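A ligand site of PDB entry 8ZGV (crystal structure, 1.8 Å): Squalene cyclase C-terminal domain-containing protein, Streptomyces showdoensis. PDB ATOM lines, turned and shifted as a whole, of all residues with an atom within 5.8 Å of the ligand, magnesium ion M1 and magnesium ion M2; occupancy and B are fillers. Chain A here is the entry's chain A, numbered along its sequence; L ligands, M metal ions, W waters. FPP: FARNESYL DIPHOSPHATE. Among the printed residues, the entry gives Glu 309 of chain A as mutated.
NE2 of Gln 169 lies within hydrogen-bond range of O1B of the ligand (2.7 Å). O2B of the ligand sits close to N of Arg 507 (2.9 Å). The side-chain amino group (NZ) of Lys 139 is in salt-bridge range of an oxygen (O2B) of the ligand (2.7 Å). NH2 of Arg 138 lies within salt-bridge range of O3B of the ligand (3.8 Å). An oxygen (O2B) of the ligand is in salt-bridge range of the guanidinium group (NE) of Arg 507 (3.5 Å).
The side-chain carboxylate of Asp 310 lies close to the backbone NH of Phe 261, at 3.3 Å. OD2 of Asp 307 is in hydrogen-bond range of N of Glu 309, 3.0 Å away. The side-chain carboxylate (OD2) of Asp 310 lies close to the backbone NH (N) of Phe 299 (3.5 Å). The backbone carbonyl oxygen (O) of Trp 399 sits at hydrogen-bond distance from the backbone NH (N) of Ala 504. O of Gly 505 lies within hydrogen-bond range of NH2 of Arg 53 (2.9 Å). SD of Met 258 lies within hydrogen-bond range of OH of Tyr 511 (3.6 Å). The indole nitrogen (NE1) of Trp 399 is in hydrogen-bond range of the side-chain hydroxyl (OG1) of Thr 349 (3.0 Å). NZ of Lys 139 is in hydrogen-bond range of O of Arg 507 (2.9 Å).
Residues that only touch the ligand: Trp 171, Asn 214, Ile 255, Met 258, Phe 261, Phe 299, Asp 307, Glu 309, Asp 310, Trp 399, Gln 503, Gly 505, Pro 506 and Tyr 511. Hydrophobic or aromatic side chains within 4 Å of the ligand: Trp 171, Ile 255, Met 258, Phe 261, Phe 299, Trp 399, Pro 506 and Tyr 511. Of the 29 residues printed, 18 come within 4 Å of the ligand. The nearest printed residue that does not touch the ligand is Phe 350 (4.05 Å).
Met 142 touches magnesium ion M1 (CE to MG, 3.9 Å). Gln 169 touches magnesium ion M1. CD1 of Leu 172 touches magnesium ion M1 (3.9 Å). Pro 506 touches magnesium ion M1. Five residues have an atom within 4 Å of magnesium ion M1: Met 142, Gln 169, Leu 172, Glu 175 and Pro 506. The nearest printed residue that does not touch magnesium ion M1 is Trp 171 (4.9 Å).
Asn 214 touches magnesium ion M2 (ND2 to MG, 3.1 Å). Two residues have an atom within 4 Å of magnesium ion M2: Glu 175 and Asn 214. Along chain A the residues within 4 Å of magnesium ion M2 span positions 175 to 214.
Magnesium ion M1 is bound by O1A of the ligand (2.5 Å). OE1 of Glu 175 binds magnesium ion M1. Magnesium ion M1 has two donor atoms within binding distance.
Magnesium ion M2 is bound by the side-chain carboxylate (OE2) of Glu 175.
Water W1 lies within hydrogen-bond range of the backbone carbonyl oxygen of Ala 504 (2.7 Å), the side-chain hydroxyl of Tyr 511 (3.0 Å) and the side-chain amide oxygen of Gln 503 (3.0 Å). Water W3 lies within hydrogen-bond range of the backbone carbonyl oxygen of Glu 212 (2.8 Å) and the side-chain amide nitrogen of Asn 214 (3.0 Å). Water W2 lies within hydrogen-bond range of the side-chain carboxylate (OD1) of Asp 307 (2.7 Å) and the backbone NH (N) of Phe 299 (3.3 Å).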
ATOM      1  N   ARG A  53      -4.762  -2.935  22.004  1.00  0.00           N
ATOM      2  CA  ARG A  53      -5.817  -2.430  22.879  1.00  0.00           C
ATOM      3  C   ARG A  53      -7.176  -2.723  22.259  1.00  0.00           C
ATOM      4  O   ARG A  53      -7.361  -2.654  21.052  1.00  0.00           O
ATOM      5  CB  ARG A  53      -5.720  -0.909  23.152  1.00  0.00           C
ATOM      6  CG  ARG A  53      -6.733  -0.437  24.166  1.00  0.00           C
ATOM      7  CD  ARG A  53      -6.293   0.832  24.904  1.00  0.00           C
ATOM      8  NE  ARG A  53      -6.429   2.018  24.064  1.00  0.00           N
ATOM      9  CZ  ARG A  53      -6.422   3.251  24.550  1.00  0.00           C
ATOM     10  NH1 ARG A  53      -6.262   3.477  25.856  1.00  0.00           N
ATOM     11  NH2 ARG A  53      -6.552   4.285  23.729  1.00  0.00           N
ATOM     12  N   ARG A 138     -17.641  16.030  28.470  1.00  0.00           N
ATOM     13  CA  ARG A 138     -17.036  15.901  27.110  1.00  0.00           C
ATOM     14  C   ARG A 138     -16.610  14.447  26.887  1.00  0.00           C
ATOM     15  O   ARG A 138     -16.832  13.935  25.809  1.00  0.00           O
ATOM     16  CB  ARG A 138     -15.850  16.855  26.972  1.00  0.00           C
ATOM     17  CG  ARG A 138     -15.121  16.795  25.629  1.00  0.00           C
ATOM     18  CD  ARG A 138     -14.358  15.504  25.375  1.00  0.00           C
ATOM     19  NE  ARG A 138     -12.910  15.528  25.550  1.00  0.00           N
ATOM     20  CZ  ARG A 138     -12.284  15.842  26.684  1.00  0.00           C
ATOM     21  NH1 ARG A 138     -12.974  16.196  27.756  1.00  0.00           N
ATOM     22  NH2 ARG A 138     -10.961  15.817  26.732  1.00  0.00           N
ATOM     23  N   LYS A 139     -15.969  13.851  27.891  1.00  0.00           N
ATOM     24  CA  LYS A 139     -15.560  12.433  27.790  1.00  0.00           C
ATOM     25  C   LYS A 139     -16.843  11.598  27.713  1.00  0.00           C
ATOM     26  O   LYS A 139     -16.860  10.627  26.966  1.00  0.00           O
ATOM     27  CB  LYS A 139     -14.724  11.993  28.996  1.00  0.00           C
ATOM     28  CG  LYS A 139     -13.252  11.782  28.718  1.00  0.00           C
ATOM     29  CD  LYS A 139     -12.390  11.919  29.951  1.00  0.00           C
ATOM     30  CE  LYS A 139     -10.964  12.331  29.637  1.00  0.00           C
ATOM     31  NZ  LYS A 139     -10.569  11.916  28.266  1.00  0.00           N
ATOM     32  N   MET A 142     -17.939  11.965  24.197  1.00  0.00           N
ATOM     33  CA  MET A 142     -17.088  11.190  23.296  1.00  0.00           C
ATOM     34  C   MET A 142     -17.375   9.692  23.420  1.00  0.00           C
ATOM     35  O   MET A 142     -17.587   9.001  22.422  1.00  0.00           O
ATOM     36  CB  MET A 142     -15.608  11.520  23.566  1.00  0.00           C
ATOM     37  CG  MET A 142     -14.615  10.639  22.790  1.00  0.00           C
ATOM     38  SD  MET A 142     -12.935  10.542  23.531  1.00  0.00           S
ATOM     39  CE  MET A 142     -12.077  11.462  22.274  1.00  0.00           C
ATOM     40  N   GLN A 169      -6.382  19.215  22.798  1.00  0.00           N
ATOM     41  CA  GLN A 169      -5.402  18.532  21.949  1.00  0.00           C
ATOM     42  C   GLN A 169      -5.783  18.812  20.474  1.00  0.00           C
ATOM     43  O   GLN A 169      -6.968  18.893  20.128  1.00  0.00           O
ATOM     44  CB  GLN A 169      -5.373  16.993  22.226  1.00  0.00           C
ATOM     45  CG  GLN A 169      -5.078  16.666  23.628  1.00  0.00           C
ATOM     46  CD  GLN A 169      -6.091  15.719  24.220  1.00  0.00           C
ATOM     47  OE1 GLN A 169      -6.345  14.637  23.680  1.00  0.00           O
ATOM     48  NE2 GLN A 169      -6.726  16.150  25.313  1.00  0.00           N
ATOM     49  N   TRP A 171      -5.205  16.307  18.888  1.00  0.00           N
ATOM     50  CA  TRP A 171      -5.727  14.937  18.826  1.00  0.00           C
ATOM     51  C   TRP A 171      -7.193  14.891  19.198  1.00  0.00           C
ATOM     52  O   TRP A 171      -8.010  14.299  18.477  1.00  0.00           O
ATOM     53  CB  TRP A 171      -4.924  14.012  19.752  1.00  0.00           C
ATOM     54  CG  TRP A 171      -3.466  14.198  19.698  1.00  0.00           C
ATOM     55  CD1 TRP A 171      -2.728  14.614  18.619  1.00  0.00           C
ATOM     56  CD2 TRP A 171      -2.530  13.974  20.763  1.00  0.00           C
ATOM     57  NE1 TRP A 171      -1.395  14.646  18.952  1.00  0.00           N
ATOM     58  CE2 TRP A 171      -1.253  14.277  20.263  1.00  0.00           C
ATOM     59  CE3 TRP A 171      -2.654  13.563  22.090  1.00  0.00           C
ATOM     60  CZ2 TRP A 171      -0.101  14.159  21.050  1.00  0.00           C
ATOM     61  CZ3 TRP A 171      -1.511  13.445  22.874  1.00  0.00           C
ATOM     62  CH2 TRP A 171      -0.247  13.751  22.356  1.00  0.00           C
ATOM     63  N   LEU A 172      -7.566  15.509  20.313  1.00  0.00           N
ATOM     64  CA  LEU A 172      -8.971  15.490  20.738  1.00  0.00           C
ATOM     65  C   LEU A 172      -9.835  16.204  19.703  1.00  0.00           C
ATOM     66  O   LEU A 172     -10.961  15.790  19.425  1.00  0.00           O
ATOM     67  CB  LEU A 172      -9.110  16.137  22.122  1.00  0.00           C
ATOM     68  CG  LEU A 172     -10.538  16.236  22.673  1.00  0.00           C
ATOM     69  CD1 LEU A 172     -11.115  14.827  22.898  1.00  0.00           C
ATOM     70  CD2 LEU A 172     -10.573  17.117  23.925  1.00  0.00           C
ATOM     71  N   GLU A 175     -10.567  13.830  16.890  1.00  0.00           N
ATOM     72  CA  GLU A 175     -11.501  12.807  17.352  1.00  0.00           C
ATOM     73  C   GLU A 175     -12.910  13.370  17.509  1.00  0.00           C
ATOM     74  O   GLU A 175     -13.878  12.741  17.088  1.00  0.00           O
ATOM     75  CB  GLU A 175     -11.013  12.209  18.679  1.00  0.00           C
ATOM     76  CG  GLU A 175      -9.616  11.537  18.488  1.00  0.00           C
ATOM     77  CD  GLU A 175      -8.877  11.238  19.768  1.00  0.00           C
ATOM     78  OE1 GLU A 175      -9.219  11.816  20.825  1.00  0.00           O
ATOM     79  OE2 GLU A 175      -7.866  10.471  19.679  1.00  0.00           O
ATOM     80  N   GLU A 212       0.375  11.612  14.148  1.00  0.00           N
ATOM     81  CA  GLU A 212       0.676  11.763  15.578  1.00  0.00           C
ATOM     82  C   GLU A 212       0.724  10.422  16.316  1.00  0.00           C
ATOM     83  O   GLU A 212       0.505  10.378  17.521  1.00  0.00           O
ATOM     84  CB  GLU A 212      -0.333  12.703  16.250  1.00  0.00           C
ATOM     85  CG  GLU A 212      -0.314  14.130  15.731  1.00  0.00           C
ATOM     86  CD  GLU A 212       0.939  14.845  16.137  1.00  0.00           C
ATOM     87  OE1 GLU A 212       1.950  14.743  15.413  1.00  0.00           O
ATOM     88  OE2 GLU A 212       0.907  15.468  17.224  1.00  0.00           O
ATOM     89  N   CYS A 213       1.023   9.342  15.592  1.00  0.00           N
ATOM     90  CA  CYS A 213       1.075   7.977  16.122  1.00  0.00           C
ATOM     91  C   CYS A 213      -0.196   7.576  16.859  1.00  0.00           C
ATOM     92  O   CYS A 213      -0.148   6.721  17.742  1.00  0.00           O
ATOM     93  CB  CYS A 213       2.290   7.761  17.034  1.00  0.00           C
ATOM     94  SG  CYS A 213       3.806   8.208  16.212  1.00  0.00           S
ATOM     95  N   ASN A 214      -1.348   8.145  16.487  1.00  0.00           N
ATOM     96  CA  ASN A 214      -2.581   8.046  17.261  1.00  0.00           C
ATOM     97  C   ASN A 214      -3.559   7.181  16.477  1.00  0.00           C
ATOM     98  O   ASN A 214      -4.253   7.672  15.585  1.00  0.00           O
ATOM     99  CB  ASN A 214      -3.171   9.417  17.525  1.00  0.00           C
ATOM    100  CG  ASN A 214      -4.202   9.393  18.605  1.00  0.00           C
ATOM    101  OD1 ASN A 214      -5.156   8.595  18.563  1.00  0.00           O
ATOM    102  ND2 ASN A 214      -4.038  10.267  19.599  1.00  0.00           N
ATOM    103  N   LEU A 216      -6.326   5.729  17.504  1.00  0.00           N
ATOM    104  CA  LEU A 216      -7.742   6.043  17.753  1.00  0.00           C
ATOM    105  C   LEU A 216      -8.224   7.166  16.848  1.00  0.00           C
ATOM    106  O   LEU A 216      -9.314   7.101  16.258  1.00  0.00           O
ATOM    107  CB  LEU A 216      -7.958   6.433  19.215  1.00  0.00           C
ATOM    108  CG  LEU A 216      -9.391   6.924  19.533  1.00  0.00           C
ATOM    109  CD1 LEU A 216     -10.422   5.814  19.243  1.00  0.00           C
ATOM    110  CD2 LEU A 216      -9.430   7.365  20.996  1.00  0.00           C
ATOM    111  N   ALA A 217      -7.439   8.234  16.764  1.00  0.00           N
ATOM    112  CA  ALA A 217      -7.837   9.401  15.976  1.00  0.00           C
ATOM    113  C   ALA A 217      -7.952   9.064  14.499  1.00  0.00           C
ATOM    114  O   ALA A 217      -8.933   9.469  13.845  1.00  0.00           O
ATOM    115  CB  ALA A 217      -6.855  10.541  16.206  1.00  0.00           C
ATOM    116  N   ILE A 255      -1.099   3.198  20.197  1.00  0.00           N
ATOM    117  CA  ILE A 255      -0.133   4.151  19.631  1.00  0.00           C
ATOM    118  C   ILE A 255       1.033   3.346  19.063  1.00  0.00           C
ATOM    119  O   ILE A 255       1.202   2.174  19.394  1.00  0.00           O
ATOM    120  CB  ILE A 255       0.384   5.150  20.695  1.00  0.00           C
ATOM    121  CG1 ILE A 255       1.029   4.399  21.878  1.00  0.00           C
ATOM    122  CG2 ILE A 255      -0.789   6.071  21.184  1.00  0.00           C
ATOM    123  CD1 ILE A 255       1.488   5.363  22.994  1.00  0.00           C
ATOM    124  N   MET A 258       6.137   4.671  22.541  1.00  0.00           N
ATOM    125  CA  MET A 258       6.336   5.813  23.429  1.00  0.00           C
ATOM    126  C   MET A 258       7.827   5.975  23.666  1.00  0.00           C
ATOM    127  O   MET A 258       8.273   6.117  24.811  1.00  0.00           O
ATOM    128  CB  MET A 258       5.609   5.565  24.741  1.00  0.00           C
ATOM    129  CG  MET A 258       4.266   6.298  24.935  1.00  0.00           C
ATOM    130  SD  MET A 258       3.829   6.202  26.706  1.00  0.00           S
ATOM    131  CE  MET A 258       4.103   7.891  27.236  1.00  0.00           C
ATOM    132  N   PHE A 261       9.343   9.365  25.539  1.00  0.00           N
ATOM    133  CA  PHE A 261       9.063   9.329  26.975  1.00  0.00           C
ATOM    134  C   PHE A 261       9.924   8.282  27.661  1.00  0.00           C
ATOM    135  O   PHE A 261      10.540   8.534  28.709  1.00  0.00           O
ATOM    136  CB  PHE A 261       7.571   9.049  27.189  1.00  0.00           C
ATOM    137  CG  PHE A 261       7.148   9.025  28.641  1.00  0.00           C
ATOM    138  CD1 PHE A 261       7.113  10.204  29.368  1.00  0.00           C
ATOM    139  CD2 PHE A 261       6.772   7.847  29.252  1.00  0.00           C
ATOM    140  CE1 PHE A 261       6.702  10.204  30.706  1.00  0.00           C
ATOM    141  CE2 PHE A 261       6.352   7.847  30.585  1.00  0.00           C
ATOM    142  CZ  PHE A 261       6.312   9.006  31.302  1.00  0.00           C
ATOM    143  N   PHE A 299       5.643  12.265  22.601  1.00  0.00           N
ATOM    144  CA  PHE A 299       5.882  11.024  23.329  1.00  0.00           C
ATOM    145  C   PHE A 299       6.598   9.965  22.491  1.00  0.00           C
ATOM    146  O   PHE A 299       7.147   9.013  23.057  1.00  0.00           O
ATOM    147  CB  PHE A 299       4.535  10.480  23.893  1.00  0.00           C
ATOM    148  CG  PHE A 299       3.534  10.095  22.817  1.00  0.00           C
ATOM    149  CD1 PHE A 299       3.568   8.845  22.228  1.00  0.00           C
ATOM    150  CD2 PHE A 299       2.545  10.996  22.413  1.00  0.00           C
ATOM    151  CE1 PHE A 299       2.669   8.486  21.235  1.00  0.00           C
ATOM    152  CE2 PHE A 299       1.624  10.659  21.441  1.00  0.00           C
ATOM    153  CZ  PHE A 299       1.659   9.400  20.850  1.00  0.00           C
ATOM    154  N   ASP A 307       4.415  17.968  24.700  1.00  0.00           N
ATOM    155  CA  ASP A 307       3.673  18.007  25.959  1.00  0.00           C
ATOM    156  C   ASP A 307       4.639  18.269  27.113  1.00  0.00           C
ATOM    157  O   ASP A 307       5.831  18.021  27.013  1.00  0.00           O
ATOM    158  CB  ASP A 307       2.868  16.716  26.185  1.00  0.00           C
ATOM    159  CG  ASP A 307       3.742  15.547  26.455  1.00  0.00           C
ATOM    160  OD1 ASP A 307       4.195  14.923  25.447  1.00  0.00           O
ATOM    161  OD2 ASP A 307       4.051  15.282  27.652  1.00  0.00           O
ATOM    162  N   GLU A 309       4.876  16.783  30.068  1.00  0.00           N
ATOM    163  CA  GLU A 309       5.442  15.628  30.767  1.00  0.00           C
ATOM    164  C   GLU A 309       6.686  15.080  30.052  1.00  0.00           C
ATOM    165  O   GLU A 309       7.745  14.866  30.675  1.00  0.00           O
ATOM    166  CB  GLU A 309       4.391  14.517  30.914  1.00  0.00           C
ATOM    167  CG  GLU A 309       4.991  13.293  31.616  1.00  0.00           C
ATOM    168  CD  GLU A 309       4.030  12.605  32.554  1.00  0.00           C
ATOM    169  OE1 GLU A 309       2.813  12.578  32.234  1.00  0.00           O
ATOM    170  OE2 GLU A 309       4.487  12.100  33.606  1.00  0.00           O
ATOM    171  N   ASP A 310       6.600  14.872  28.731  1.00  0.00           N
ATOM    172  CA  ASP A 310       7.763  14.438  27.971  1.00  0.00           C
ATOM    173  C   ASP A 310       8.881  15.443  28.053  1.00  0.00           C
ATOM    174  O   ASP A 310      10.051  15.093  28.222  1.00  0.00           O
ATOM    175  CB  ASP A 310       7.411  14.218  26.490  1.00  0.00           C
ATOM    176  CG  ASP A 310       6.718  12.899  26.255  1.00  0.00           C
ATOM    177  OD1 ASP A 310       7.440  11.879  26.352  1.00  0.00           O
ATOM    178  OD2 ASP A 310       5.482  12.866  26.017  1.00  0.00           O
ATOM    179  N   THR A 349      -1.038  20.648  30.413  1.00  0.00           N
ATOM    180  CA  THR A 349      -0.344  19.521  29.798  1.00  0.00           C
ATOM    181  C   THR A 349       0.212  19.853  28.420  1.00  0.00           C
ATOM    182  O   THR A 349       1.326  19.426  28.086  1.00  0.00           O
ATOM    183  CB  THR A 349      -1.282  18.320  29.662  1.00  0.00           C
ATOM    184  OG1 THR A 349      -1.680  17.871  30.957  1.00  0.00           O
ATOM    185  CG2 THR A 349      -0.521  17.194  28.939  1.00  0.00           C
ATOM    186  N   PHE A 350      -0.568  20.574  27.595  1.00  0.00           N
ATOM    187  CA  PHE A 350      -0.247  20.849  26.197  1.00  0.00           C
ATOM    188  C   PHE A 350      -0.261  22.332  25.870  1.00  0.00           C
ATOM    189  O   PHE A 350       0.620  22.818  25.147  1.00  0.00           O
ATOM    190  CB  PHE A 350      -1.286  20.237  25.229  1.00  0.00           C
ATOM    191  CG  PHE A 350      -1.436  18.766  25.302  1.00  0.00           C
ATOM    192  CD1 PHE A 350      -0.481  17.919  24.755  1.00  0.00           C
ATOM    193  CD2 PHE A 350      -2.560  18.212  25.891  1.00  0.00           C
ATOM    194  CE1 PHE A 350      -0.630  16.552  24.797  1.00  0.00           C
ATOM    195  CE2 PHE A 350      -2.732  16.845  25.956  1.00  0.00           C
ATOM    196  CZ  PHE A 350      -1.755  16.001  25.410  1.00  0.00           C
ATOM    197  N   TRP A 399      -2.848  11.628  33.868  1.00  0.00           N
ATOM    198  CA  TRP A 399      -2.250  10.723  32.899  1.00  0.00           C
ATOM    199  C   TRP A 399      -1.837   9.386  33.514  1.00  0.00           C
ATOM    200  O   TRP A 399      -1.739   8.399  32.783  1.00  0.00           O
ATOM    201  CB  TRP A 399      -1.061  11.413  32.241  1.00  0.00           C
ATOM    202  CG  TRP A 399      -1.505  12.659  31.518  1.00  0.00           C
ATOM    203  CD1 TRP A 399      -1.111  13.953  31.771  1.00  0.00           C
ATOM    204  CD2 TRP A 399      -2.457  12.740  30.428  1.00  0.00           C
ATOM    205  NE1 TRP A 399      -1.744  14.826  30.910  1.00  0.00           N
ATOM    206  CE2 TRP A 399      -2.564  14.110  30.072  1.00  0.00           C
ATOM    207  CE3 TRP A 399      -3.202  11.800  29.719  1.00  0.00           C
ATOM    208  CZ2 TRP A 399      -3.410  14.551  29.038  1.00  0.00           C
ATOM    209  CZ3 TRP A 399      -4.039  12.242  28.691  1.00  0.00           C
ATOM    210  CH2 TRP A 399      -4.128  13.605  28.365  1.00  0.00           C
ATOM    211  N   GLN A 503      -0.437   4.084  32.332  1.00  0.00           N
ATOM    212  CA  GLN A 503      -0.672   5.168  31.382  1.00  0.00           C
ATOM    213  C   GLN A 503      -2.095   5.108  30.829  1.00  0.00           C
ATOM    214  O   GLN A 503      -2.578   4.039  30.474  1.00  0.00           O
ATOM    215  CB  GLN A 503       0.306   5.113  30.212  1.00  0.00           C
ATOM    216  CG  GLN A 503       1.801   5.148  30.603  1.00  0.00           C
ATOM    217  CD  GLN A 503       2.216   6.492  31.097  1.00  0.00           C
ATOM    218  OE1 GLN A 503       1.889   7.505  30.488  1.00  0.00           O
ATOM    219  NE2 GLN A 503       2.989   6.508  32.182  1.00  0.00           N
ATOM    220  N   ALA A 504      -2.749   6.262  30.745  1.00  0.00           N
ATOM    221  CA  ALA A 504      -4.098   6.362  30.194  1.00  0.00           C
ATOM    222  C   ALA A 504      -4.143   7.391  29.071  1.00  0.00           C
ATOM    223  O   ALA A 504      -3.364   8.352  29.027  1.00  0.00           O
ATOM    224  CB  ALA A 504      -5.112   6.724  31.261  1.00  0.00           C
ATOM    225  N   GLY A 505      -5.088   7.190  28.162  1.00  0.00           N
ATOM    226  CA  GLY A 505      -5.319   8.110  27.083  1.00  0.00           C
ATOM    227  C   GLY A 505      -6.132   7.442  26.006  1.00  0.00           C
ATOM    228  O   GLY A 505      -5.793   6.359  25.536  1.00  0.00           O
ATOM    229  N   PRO A 506      -7.284   8.037  25.655  1.00  0.00           N
ATOM    230  CA  PRO A 506      -7.975   9.123  26.375  1.00  0.00           C
ATOM    231  C   PRO A 506      -8.271   8.697  27.799  1.00  0.00           C
ATOM    232  O   PRO A 506      -8.713   7.569  28.007  1.00  0.00           O
ATOM    233  CB  PRO A 506      -9.298   9.288  25.613  1.00  0.00           C
ATOM    234  CG  PRO A 506      -9.096   8.578  24.308  1.00  0.00           C
ATOM    235  CD  PRO A 506      -8.136   7.459  24.605  1.00  0.00           C
ATOM    236  N   ARG A 507      -8.083   9.593  28.767  1.00  0.00           N
ATOM    237  CA  ARG A 507      -8.345   9.218  30.145  1.00  0.00           C
ATOM    238  C   ARG A 507      -9.790   8.754  30.255  1.00  0.00           C
ATOM    239  O   ARG A 507     -10.678   9.333  29.605  1.00  0.00           O
ATOM    240  CB  ARG A 507      -8.153  10.417  31.087  1.00  0.00           C
ATOM    241  CG  ARG A 507      -6.793  11.058  31.154  1.00  0.00           C
ATOM    242  CD  ARG A 507      -7.044  12.555  30.963  1.00  0.00           C
ATOM    243  NE  ARG A 507      -5.855  13.390  30.981  1.00  0.00           N
ATOM    244  CZ  ARG A 507      -5.675  14.371  31.871  1.00  0.00           C
ATOM    245  NH1 ARG A 507      -6.601  14.669  32.770  1.00  0.00           N
ATOM    246  NH2 ARG A 507      -4.546  15.055  31.863  1.00  0.00           N
ATOM    247  N   TYR A 511      -3.478   2.108  28.519  1.00  0.00           N
ATOM    248  CA  TYR A 511      -2.807   1.405  27.438  1.00  0.00           C
ATOM    249  C   TYR A 511      -1.476   0.928  28.005  1.00  0.00           C
ATOM    250  O   TYR A 511      -1.019   1.429  29.042  1.00  0.00           O
ATOM    251  CB  TYR A 511      -2.600   2.258  26.163  1.00  0.00           C
ATOM    252  CG  TYR A 511      -1.800   3.514  26.392  1.00  0.00           C
ATOM    253  CD1 TYR A 511      -0.417   3.510  26.255  1.00  0.00           C
ATOM    254  CD2 TYR A 511      -2.447   4.701  26.712  1.00  0.00           C
ATOM    255  CE1 TYR A 511       0.323   4.657  26.496  1.00  0.00           C
ATOM    256  CE2 TYR A 511      -1.743   5.853  26.914  1.00  0.00           C
ATOM    257  CZ  TYR A 511      -0.359   5.843  26.798  1.00  0.00           C
ATOM    258  OH  TYR A 511       0.345   6.995  27.000  1.00  0.00           O
HETATM  259  C1  FPP L   1      -4.842   9.470  23.789  1.00  0.00           C
HETATM  260  O1  FPP L   1      -4.544  10.254  24.922  1.00  0.00           O
HETATM  261  C2  FPP L   1      -3.702   8.464  23.616  1.00  0.00           C
HETATM  262  C3  FPP L   1      -2.377   9.211  23.658  1.00  0.00           C
HETATM  263  C4  FPP L   1      -1.620   9.229  22.322  1.00  0.00           C
HETATM  264  C5  FPP L   1      -1.550   8.828  24.880  1.00  0.00           C
HETATM  265  C6  FPP L   1      -1.244  10.070  25.706  1.00  0.00           C
HETATM  266  C7  FPP L   1       0.146  10.601  25.323  1.00  0.00           C
HETATM  267  C8  FPP L   1       0.741  11.708  26.207  1.00  0.00           C
HETATM  268  C10 FPP L   1       1.329  12.909  25.463  1.00  0.00           C
HETATM  269  C9  FPP L   1      -0.106  12.114  27.408  1.00  0.00           C
HETATM  270  C11 FPP L   1       0.351  11.308  28.631  1.00  0.00           C
HETATM  271  C12 FPP L   1       1.745  11.777  29.062  1.00  0.00           C
HETATM  272  C13 FPP L   1       2.837  10.737  28.830  1.00  0.00           C
HETATM  273  C14 FPP L   1       3.231   9.952  30.088  1.00  0.00           C
HETATM  274  C15 FPP L   1       4.036  11.326  28.091  1.00  0.00           C
HETATM  275  PA  FPP L   1      -5.241  11.749  25.167  1.00  0.00           P
HETATM  276  O1A FPP L   1      -5.981  12.156  23.950  1.00  0.00           O
HETATM  277  O2A FPP L   1      -4.197  12.778  25.304  1.00  0.00           O
HETATM  278  O3A FPP L   1      -6.165  11.722  26.546  1.00  0.00           O
HETATM  279  PB  FPP L   1      -7.333  12.829  27.012  1.00  0.00           P
HETATM  280  O1B FPP L   1      -6.844  14.216  27.183  1.00  0.00           O
HETATM  281  O2B FPP L   1      -7.954  12.497  28.276  1.00  0.00           O
HETATM  282  O3B FPP L   1      -8.459  12.977  26.061  1.00  0.00           O
HETATM  283 MG    MG M   1      -8.320  12.109  23.123  1.00  0.00          MG
HETATM  284 MG    MG M   2      -6.289   9.906  21.666  1.00  0.00          MG
HETATM  285  O   HOH W   1      -0.647   8.607  29.319  1.00  0.00           O
HETATM  286  O   HOH W   2       3.115  14.374  23.011  1.00  0.00           O
HETATM  287  O   HOH W   3      -1.213  11.163  19.595  1.00  0.00           O
